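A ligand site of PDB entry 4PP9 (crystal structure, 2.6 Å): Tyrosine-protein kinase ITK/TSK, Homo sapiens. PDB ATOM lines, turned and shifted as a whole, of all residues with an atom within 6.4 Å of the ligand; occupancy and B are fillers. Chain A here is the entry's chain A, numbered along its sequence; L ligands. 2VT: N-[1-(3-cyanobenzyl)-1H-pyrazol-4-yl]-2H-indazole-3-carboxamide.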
ATOM      1  N   GLN A  13      -0.121 -27.187  -8.753  1.00  0.00           N
ATOM      2  CA  GLN A  13       0.256 -28.158  -7.716  1.00  0.00           C
ATOM      3  C   GLN A  13      -0.884 -29.117  -7.329  1.00  0.00           C
ATOM      4  O   GLN A  13      -2.050 -28.836  -7.599  1.00  0.00           O
ATOM      5  CB  GLN A  13       0.843 -27.458  -6.465  1.00  0.00           C
ATOM      6  CG  GLN A  13      -0.153 -26.699  -5.590  1.00  0.00           C
ATOM      7  CD  GLN A  13       0.571 -25.853  -4.576  1.00  0.00           C
ATOM      8  OE1 GLN A  13       0.765 -24.657  -4.780  1.00  0.00           O
ATOM      9  NE2 GLN A  13       0.990 -26.469  -3.469  1.00  0.00           N
ATOM     10  N   GLU A  14      -0.537 -30.248  -6.675  1.00  0.00           N
ATOM     11  CA  GLU A  14      -1.455 -31.278  -6.180  1.00  0.00           C
ATOM     12  C   GLU A  14      -1.906 -30.840  -4.768  1.00  0.00           C
ATOM     13  O   GLU A  14      -1.065 -30.512  -3.942  1.00  0.00           O
ATOM     14  CB  GLU A  14      -0.715 -32.625  -6.116  1.00  0.00           C
ATOM     15  CG  GLU A  14      -1.554 -33.819  -6.514  1.00  0.00           C
ATOM     16  CD  GLU A  14      -0.755 -35.019  -6.990  1.00  0.00           C
ATOM     17  OE1 GLU A  14       0.246 -35.372  -6.337  1.00  0.00           O
ATOM     18  OE2 GLU A  14      -1.153 -35.618  -8.024  1.00  0.00           O
ATOM     19  N   ILE A  15      -3.219 -30.768  -4.533  1.00  0.00           N
ATOM     20  CA  ILE A  15      -3.751 -30.256  -3.253  1.00  0.00           C
ATOM     21  C   ILE A  15      -4.679 -31.242  -2.498  1.00  0.00           C
ATOM     22  O   ILE A  15      -5.081 -30.944  -1.361  1.00  0.00           O
ATOM     23  CB  ILE A  15      -4.412 -28.843  -3.423  1.00  0.00           C
ATOM     24  CG1 ILE A  15      -5.586 -28.864  -4.435  1.00  0.00           C
ATOM     25  CG2 ILE A  15      -3.363 -27.762  -3.769  1.00  0.00           C
ATOM     26  CD1 ILE A  15      -6.517 -27.664  -4.370  1.00  0.00           C
ATOM     27  N   GLY A  16      -4.979 -32.381  -3.101  1.00  0.00           N
ATOM     28  CA  GLY A  16      -5.832 -33.392  -2.493  1.00  0.00           C
ATOM     29  C   GLY A  16      -6.051 -34.641  -3.323  1.00  0.00           C
ATOM     30  O   GLY A  16      -5.942 -34.604  -4.546  1.00  0.00           O
ATOM     31  N   VAL A  23      -7.321 -33.697  -6.760  1.00  0.00           N
ATOM     32  CA  VAL A  23      -7.616 -32.277  -6.825  1.00  0.00           C
ATOM     33  C   VAL A  23      -6.289 -31.499  -6.954  1.00  0.00           C
ATOM     34  O   VAL A  23      -5.334 -31.788  -6.239  1.00  0.00           O
ATOM     35  CB  VAL A  23      -8.521 -31.777  -5.654  1.00  0.00           C
ATOM     36  CG1 VAL A  23      -8.839 -30.292  -5.779  1.00  0.00           C
ATOM     37  CG2 VAL A  23      -9.806 -32.586  -5.574  1.00  0.00           C
ATOM     38  N   LEU A  25      -4.441 -27.441  -7.740  1.00  0.00           N
ATOM     39  CA  LEU A  25      -4.551 -25.992  -7.754  1.00  0.00           C
ATOM     40  C   LEU A  25      -4.044 -25.596  -9.141  1.00  0.00           C
ATOM     41  O   LEU A  25      -2.946 -25.998  -9.535  1.00  0.00           O
ATOM     42  CB  LEU A  25      -3.690 -25.316  -6.649  1.00  0.00           C
ATOM     43  CG  LEU A  25      -3.220 -23.848  -6.887  1.00  0.00           C
ATOM     44  CD1 LEU A  25      -4.371 -22.866  -6.825  1.00  0.00           C
ATOM     45  CD2 LEU A  25      -2.162 -23.445  -5.895  1.00  0.00           C
ATOM     46  N   LYS A  33      -8.183 -18.556 -10.617  1.00  0.00           N
ATOM     47  CA  LYS A  33      -7.598 -19.573  -9.749  1.00  0.00           C
ATOM     48  C   LYS A  33      -8.645 -20.655  -9.613  1.00  0.00           C
ATOM     49  O   LYS A  33      -9.783 -20.374  -9.215  1.00  0.00           O
ATOM     50  CB  LYS A  33      -7.228 -18.975  -8.382  1.00  0.00           C
ATOM     51  CG  LYS A  33      -6.039 -19.629  -7.713  1.00  0.00           C
ATOM     52  CD  LYS A  33      -5.862 -19.083  -6.298  1.00  0.00           C
ATOM     53  CE  LYS A  33      -4.468 -19.267  -5.759  1.00  0.00           C
ATOM     54  NZ  LYS A  33      -4.236 -18.404  -4.564  1.00  0.00           N
ATOM     55  N   VAL A  34      -8.302 -21.877 -10.003  1.00  0.00           N
ATOM     56  CA  VAL A  34      -9.257 -22.994  -9.983  1.00  0.00           C
ATOM     57  C   VAL A  34      -8.768 -24.206  -9.179  1.00  0.00           C
ATOM     58  O   VAL A  34      -7.598 -24.288  -8.776  1.00  0.00           O
ATOM     59  CB  VAL A  34      -9.711 -23.417 -11.420  1.00  0.00           C
ATOM     60  CG1 VAL A  34     -10.441 -22.285 -12.138  1.00  0.00           C
ATOM     61  CG2 VAL A  34      -8.551 -23.947 -12.265  1.00  0.00           C
ATOM     62  N   ALA A  35      -9.699 -25.129  -8.948  1.00  0.00           N
ATOM     63  CA  ALA A  35      -9.479 -26.420  -8.329  1.00  0.00           C
ATOM     64  C   ALA A  35      -9.925 -27.401  -9.415  1.00  0.00           C
ATOM     65  O   ALA A  35     -11.071 -27.344  -9.886  1.00  0.00           O
ATOM     66  CB  ALA A  35     -10.312 -26.577  -7.083  1.00  0.00           C
ATOM     67  N   LYS A  37     -10.533 -31.196 -10.526  1.00  0.00           N
ATOM     68  CA  LYS A  37     -10.823 -32.519  -9.982  1.00  0.00           C
ATOM     69  C   LYS A  37     -10.737 -33.554 -11.098  1.00  0.00           C
ATOM     70  O   LYS A  37     -11.698 -33.764 -11.838  1.00  0.00           O
ATOM     71  CB  LYS A  37     -12.189 -32.522  -9.270  1.00  0.00           C
ATOM     72  CG  LYS A  37     -12.437 -33.758  -8.403  1.00  0.00           C
ATOM     73  CD  LYS A  37     -13.623 -33.568  -7.461  1.00  0.00           C
ATOM     74  CE  LYS A  37     -13.785 -34.709  -6.489  1.00  0.00           C
ATOM     75  NZ  LYS A  37     -14.852 -34.444  -5.489  1.00  0.00           N
ATOM     76  N   VAL A  65     -20.768 -24.869  -3.645  1.00  0.00           N
ATOM     77  CA  VAL A  65     -19.626 -24.716  -4.568  1.00  0.00           C
ATOM     78  C   VAL A  65     -20.096 -24.529  -6.026  1.00  0.00           C
ATOM     79  O   VAL A  65     -21.130 -25.075  -6.416  1.00  0.00           O
ATOM     80  CB  VAL A  65     -18.583 -25.863  -4.416  1.00  0.00           C
ATOM     81  CG1 VAL A  65     -19.053 -27.170  -5.065  1.00  0.00           C
ATOM     82  CG2 VAL A  65     -17.212 -25.451  -4.957  1.00  0.00           C
ATOM     83  N   GLN A  66     -19.335 -23.748  -6.811  1.00  0.00           N
ATOM     84  CA  GLN A  66     -19.634 -23.460  -8.213  1.00  0.00           C
ATOM     85  C   GLN A  66     -18.538 -23.986  -9.136  1.00  0.00           C
ATOM     86  O   GLN A  66     -17.361 -23.990  -8.768  1.00  0.00           O
ATOM     87  CB  GLN A  66     -19.810 -21.960  -8.438  1.00  0.00           C
ATOM     88  CG  GLN A  66     -20.915 -21.344  -7.600  1.00  0.00           C
ATOM     89  CD  GLN A  66     -21.214 -19.938  -8.063  1.00  0.00           C
ATOM     90  OE1 GLN A  66     -22.187 -19.710  -8.788  1.00  0.00           O
ATOM     91  NE2 GLN A  66     -20.369 -18.992  -7.670  1.00  0.00           N
ATOM     92  N   PHE A  81     -13.583 -26.500 -10.872  1.00  0.00           N
ATOM     93  CA  PHE A  81     -14.360 -25.758  -9.882  1.00  0.00           C
ATOM     94  C   PHE A  81     -13.703 -24.443  -9.515  1.00  0.00           C
ATOM     95  O   PHE A  81     -12.536 -24.223  -9.838  1.00  0.00           O
ATOM     96  CB  PHE A  81     -14.481 -26.588  -8.583  1.00  0.00           C
ATOM     97  CG  PHE A  81     -15.191 -27.911  -8.654  1.00  0.00           C
ATOM     98  CD1 PHE A  81     -14.494 -29.077  -8.955  1.00  0.00           C
ATOM     99  CD2 PHE A  81     -16.535 -28.011  -8.329  1.00  0.00           C
ATOM    100  CE1 PHE A  81     -15.154 -30.311  -8.968  1.00  0.00           C
ATOM    101  CE2 PHE A  81     -17.188 -29.247  -8.349  1.00  0.00           C
ATOM    102  CZ  PHE A  81     -16.499 -30.389  -8.666  1.00  0.00           C
ATOM    103  N   GLU A  82     -14.419 -23.582  -8.766  1.00  0.00           N
ATOM    104  CA  GLU A  82     -13.867 -22.337  -8.232  1.00  0.00           C
ATOM    105  C   GLU A  82     -12.938 -22.774  -7.088  1.00  0.00           C
ATOM    106  O   GLU A  82     -13.191 -23.807  -6.457  1.00  0.00           O
ATOM    107  CB  GLU A  82     -14.986 -21.416  -7.732  1.00  0.00           C
ATOM    108  CG  GLU A  82     -15.755 -21.962  -6.526  1.00  0.00           C
ATOM    109  CD  GLU A  82     -16.846 -21.107  -5.932  1.00  0.00           C
ATOM    110  OE1 GLU A  82     -16.628 -19.889  -5.735  1.00  0.00           O
ATOM    111  OE2 GLU A  82     -17.901 -21.678  -5.575  1.00  0.00           O
ATOM    112  N   PHE A  83     -11.852 -22.035  -6.862  1.00  0.00           N
ATOM    113  CA  PHE A  83     -10.903 -22.384  -5.802  1.00  0.00           C
ATOM    114  C   PHE A  83     -11.394 -21.927  -4.436  1.00  0.00           C
ATOM    115  O   PHE A  83     -11.838 -20.785  -4.272  1.00  0.00           O
ATOM    116  CB  PHE A  83      -9.514 -21.806  -6.114  1.00  0.00           C
ATOM    117  CG  PHE A  83      -8.388 -22.304  -5.232  1.00  0.00           C
ATOM    118  CD1 PHE A  83      -7.873 -23.582  -5.394  1.00  0.00           C
ATOM    119  CD2 PHE A  83      -7.828 -21.478  -4.268  1.00  0.00           C
ATOM    120  CE1 PHE A  83      -6.850 -24.047  -4.564  1.00  0.00           C
ATOM    121  CE2 PHE A  83      -6.770 -21.927  -3.468  1.00  0.00           C
ATOM    122  CZ  PHE A  83      -6.296 -23.214  -3.622  1.00  0.00           C
ATOM    123  N   MET A  84     -11.336 -22.844  -3.450  1.00  0.00           N
ATOM    124  CA  MET A  84     -11.712 -22.582  -2.061  1.00  0.00           C
ATOM    125  C   MET A  84     -10.418 -22.602  -1.262  1.00  0.00           C
ATOM    126  O   MET A  84      -9.916 -23.663  -0.914  1.00  0.00           O
ATOM    127  CB  MET A  84     -12.758 -23.575  -1.543  1.00  0.00           C
ATOM    128  CG  MET A  84     -14.122 -23.430  -2.211  1.00  0.00           C
ATOM    129  SD  MET A  84     -14.919 -21.807  -2.014  1.00  0.00           S
ATOM    130  CE  MET A  84     -15.707 -22.018  -0.419  1.00  0.00           C
ATOM    131  N   GLU A  85      -9.856 -21.396  -1.075  1.00  0.00           N
ATOM    132  CA  GLU A  85      -8.566 -21.063  -0.451  1.00  0.00           C
ATOM    133  C   GLU A  85      -8.110 -21.958   0.721  1.00  0.00           C
ATOM    134  O   GLU A  85      -6.971 -22.420   0.689  1.00  0.00           O
ATOM    135  CB  GLU A  85      -8.566 -19.590  -0.026  1.00  0.00           C
ATOM    136  CG  GLU A  85      -7.225 -18.894  -0.211  1.00  0.00           C
ATOM    137  CD  GLU A  85      -6.840 -18.540  -1.643  1.00  0.00           C
ATOM    138  OE1 GLU A  85      -7.499 -17.666  -2.244  1.00  0.00           O
ATOM    139  OE2 GLU A  85      -5.835 -19.108  -2.136  1.00  0.00           O
ATOM    140  N   HIS A  86      -8.973 -22.187   1.737  1.00  0.00           N
ATOM    141  CA  HIS A  86      -8.612 -22.936   2.952  1.00  0.00           C
ATOM    142  C   HIS A  86      -8.944 -24.439   2.920  1.00  0.00           C
ATOM    143  O   HIS A  86      -8.630 -25.159   3.879  1.00  0.00           O
ATOM    144  CB  HIS A  86      -9.232 -22.261   4.202  1.00  0.00           C
ATOM    145  CG  HIS A  86      -8.839 -20.827   4.345  1.00  0.00           C
ATOM    146  ND1 HIS A  86      -7.531 -20.447   4.598  1.00  0.00           N
ATOM    147  CD2 HIS A  86      -9.595 -19.710   4.221  1.00  0.00           C
ATOM    148  CE1 HIS A  86      -7.530 -19.124   4.622  1.00  0.00           C
ATOM    149  NE2 HIS A  86      -8.750 -18.637   4.411  1.00  0.00           N
ATOM    150  N   GLY A  87      -9.491 -24.908   1.796  1.00  0.00           N
ATOM    151  CA  GLY A  87      -9.803 -26.319   1.594  1.00  0.00           C
ATOM    152  C   GLY A  87     -10.963 -26.829   2.414  1.00  0.00           C
ATOM    153  O   GLY A  87     -11.825 -26.058   2.828  1.00  0.00           O
ATOM    154  N   CYS A  88     -10.975 -28.154   2.637  1.00  0.00           N
ATOM    155  CA  CYS A  88     -12.016 -28.895   3.369  1.00  0.00           C
ATOM    156  C   CYS A  88     -12.168 -28.401   4.802  1.00  0.00           C
ATOM    157  O   CYS A  88     -11.174 -28.041   5.434  1.00  0.00           O
ATOM    158  CB  CYS A  88     -11.748 -30.398   3.338  1.00  0.00           C
ATOM    159  SG  CYS A  88     -11.271 -31.032   1.708  1.00  0.00           S
ATOM    160  N   LEU A 135     -16.316 -27.040   2.012  1.00  0.00           N
ATOM    161  CA  LEU A 135     -15.130 -26.251   1.702  1.00  0.00           C
ATOM    162  C   LEU A 135     -15.169 -24.834   2.267  1.00  0.00           C
ATOM    163  O   LEU A 135     -16.192 -24.154   2.203  1.00  0.00           O
ATOM    164  CB  LEU A 135     -14.857 -26.235   0.200  1.00  0.00           C
ATOM    165  CG  LEU A 135     -14.496 -27.591  -0.423  1.00  0.00           C
ATOM    166  CD1 LEU A 135     -15.061 -27.706  -1.807  1.00  0.00           C
ATOM    167  CD2 LEU A 135     -12.996 -27.823  -0.424  1.00  0.00           C
ATOM    168  N   VAL A 136     -14.017 -24.419   2.816  1.00  0.00           N
ATOM    169  CA  VAL A 136     -13.741 -23.123   3.426  1.00  0.00           C
ATOM    170  C   VAL A 136     -13.032 -22.260   2.377  1.00  0.00           C
ATOM    171  O   VAL A 136     -12.039 -22.701   1.784  1.00  0.00           O
ATOM    172  CB  VAL A 136     -12.870 -23.265   4.708  1.00  0.00           C
ATOM    173  CG1 VAL A 136     -12.830 -21.971   5.521  1.00  0.00           C
ATOM    174  CG2 VAL A 136     -13.336 -24.435   5.571  1.00  0.00           C
ATOM    175  N   SER A 145     -20.113 -29.132  -1.040  1.00  0.00           N
ATOM    176  CA  SER A 145     -19.657 -29.766  -2.262  1.00  0.00           C
ATOM    177  C   SER A 145     -20.101 -31.237  -2.269  1.00  0.00           C
ATOM    178  O   SER A 145     -20.605 -31.730  -1.258  1.00  0.00           O
ATOM    179  CB  SER A 145     -18.144 -29.656  -2.387  1.00  0.00           C
ATOM    180  OG  SER A 145     -17.472 -30.445  -1.418  1.00  0.00           O
ATOM    181  N   ASP A 146     -19.872 -31.947  -3.408  1.00  0.00           N
ATOM    182  CA  ASP A 146     -20.180 -33.361  -3.635  1.00  0.00           C
ATOM    183  C   ASP A 146     -21.697 -33.656  -3.490  1.00  0.00           C
ATOM    184  O   ASP A 146     -22.090 -34.642  -2.852  1.00  0.00           O
ATOM    185  CB  ASP A 146     -19.299 -34.276  -2.750  1.00  0.00           C
ATOM    186  CG  ASP A 146     -17.781 -34.125  -2.928  1.00  0.00           C
ATOM    187  OD1 ASP A 146     -17.354 -33.136  -3.577  1.00  0.00           O
ATOM    188  OD2 ASP A 146     -17.028 -34.980  -2.401  1.00  0.00           O
HETATM  189  C1  2VT L   1     -13.140 -29.928  -4.471  1.00  0.00           C
HETATM  190  C2  2VT L   1     -14.072 -29.153  -5.169  1.00  0.00           C
HETATM  191  C3  2VT L   1     -13.930 -27.785  -5.255  1.00  0.00           C
HETATM  192  C4  2VT L   1     -12.845 -27.158  -4.633  1.00  0.00           C
HETATM  193  C5  2VT L   1     -11.885 -27.958  -3.928  1.00  0.00           C
HETATM  194  C6  2VT L   1     -12.046 -29.349  -3.851  1.00  0.00           C
HETATM  195  C7  2VT L   1     -10.903 -26.979  -3.417  1.00  0.00           C
HETATM  196  N8  2VT L   1     -11.319 -25.793  -3.841  1.00  0.00           N
HETATM  197  N9  2VT L   1     -12.414 -25.865  -4.516  1.00  0.00           N
HETATM  198  C11 2VT L   1      -9.695 -27.245  -2.597  1.00  0.00           C
HETATM  199  O12 2VT L   1      -9.349 -28.402  -2.435  1.00  0.00           O
HETATM  200  N13 2VT L   1      -9.002 -26.212  -2.037  1.00  0.00           N
HETATM  201  C14 2VT L   1      -7.838 -26.344  -1.236  1.00  0.00           C
HETATM  202  C15 2VT L   1      -7.236 -27.533  -0.790  1.00  0.00           C
HETATM  203  N16 2VT L   1      -6.197 -27.245  -0.061  1.00  0.00           N
HETATM  204  N17 2VT L   1      -6.078 -25.856   0.010  1.00  0.00           N
HETATM  205  C18 2VT L   1      -7.097 -25.321  -0.714  1.00  0.00           C
HETATM  206  C19 2VT L   1      -5.036 -25.143   0.746  1.00  0.00           C
HETATM  207  C20 2VT L   1      -3.988 -24.705  -0.227  1.00  0.00           C
HETATM  208  C21 2VT L   1      -2.942 -25.565  -0.561  1.00  0.00           C
HETATM  209  C22 2VT L   1      -1.973 -25.166  -1.481  1.00  0.00           C
HETATM  210  C23 2VT L   1      -2.059 -23.904  -2.075  1.00  0.00           C
HETATM  211  C24 2VT L   1      -3.105 -23.036  -1.729  1.00  0.00           C
HETATM  212  C25 2VT L   1      -4.078 -23.449  -0.809  1.00  0.00           C
HETATM  213  C26 2VT L   1      -3.187 -21.731  -2.335  1.00  0.00           C
HETATM  214  N27 2VT L   1      -3.257 -20.701  -2.802  1.00  0.00           N
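OE2 of Glu 85 lies close to N27 of the ligand. Residues that only touch the ligand: Gln 13 (3.8 Å), Ile 15 (3.5 Å), Val 23 (3.9 Å), Leu 25 (3.8 Å), Ala 35 (3.4 Å), Phe 81 (3.6 Å), Phe 83 (3.6 Å), Gly 87 (3.4 Å) and Leu 135 (3.6 Å). Hydrophobic or aromatic side chains within 4 Å of the ligand: Ile 15, Val 23, Leu 25, Ala 35, Phe 81, Phe 83, Met 84 and Leu 135. Within 4 Å of the ligand: Gln 13, Ile 15, Val 23, Leu 25, Lys 33, Ala 35, Phe 81, Glu 82, Phe 83, Met 84, Glu 85, Gly 87 and Leu 135. The nearest printed residue that does not touch the ligand is Val 65 (4.04 Å).
N9 of the ligand sits close to O of Glu 82. A nitrogen (N9) of the ligand sits at hydrogen-bond distance from the backbone NH (N) of Met 84, 3.4 Å away. The backbone carbonyl oxygen (O) of Met 84 sits at hydrogen-bond distance from a nitrogen (N13) of the ligand (2.9 Å). A nitrogen (N27) of the ligand lies within hydrogen-bond range of the side-chain amino group of Lys 33 (3.1 Å).
The side-chain amino group (NZ) of Lys 33 is in salt-bridge range of the side-chain carboxylate (OE2) of Glu 85. The backbone carbonyl oxygen of Gln 13 sits at hydrogen-bond distance from the backbone NH of Leu 25, at 2.8 Å. The backbone carbonyl oxygen (O) of Gly 87 is in hydrogen-bond range of the backbone NH (N) of Val 136, 2.7 Å away. OE2 of Glu 82 is in hydrogen-bond range of N of Gln 66. O of Ala 35 lies within hydrogen-bond range of N of Phe 81 (2.8 Å). N of Ile 15 is in hydrogen-bond range of O of Val 23 (2.9 Å). The backbone carbonyl oxygen (O) of Gly 16 is in hydrogen-bond range of the backbone NH (N) of Val 23 (2.8 Å).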
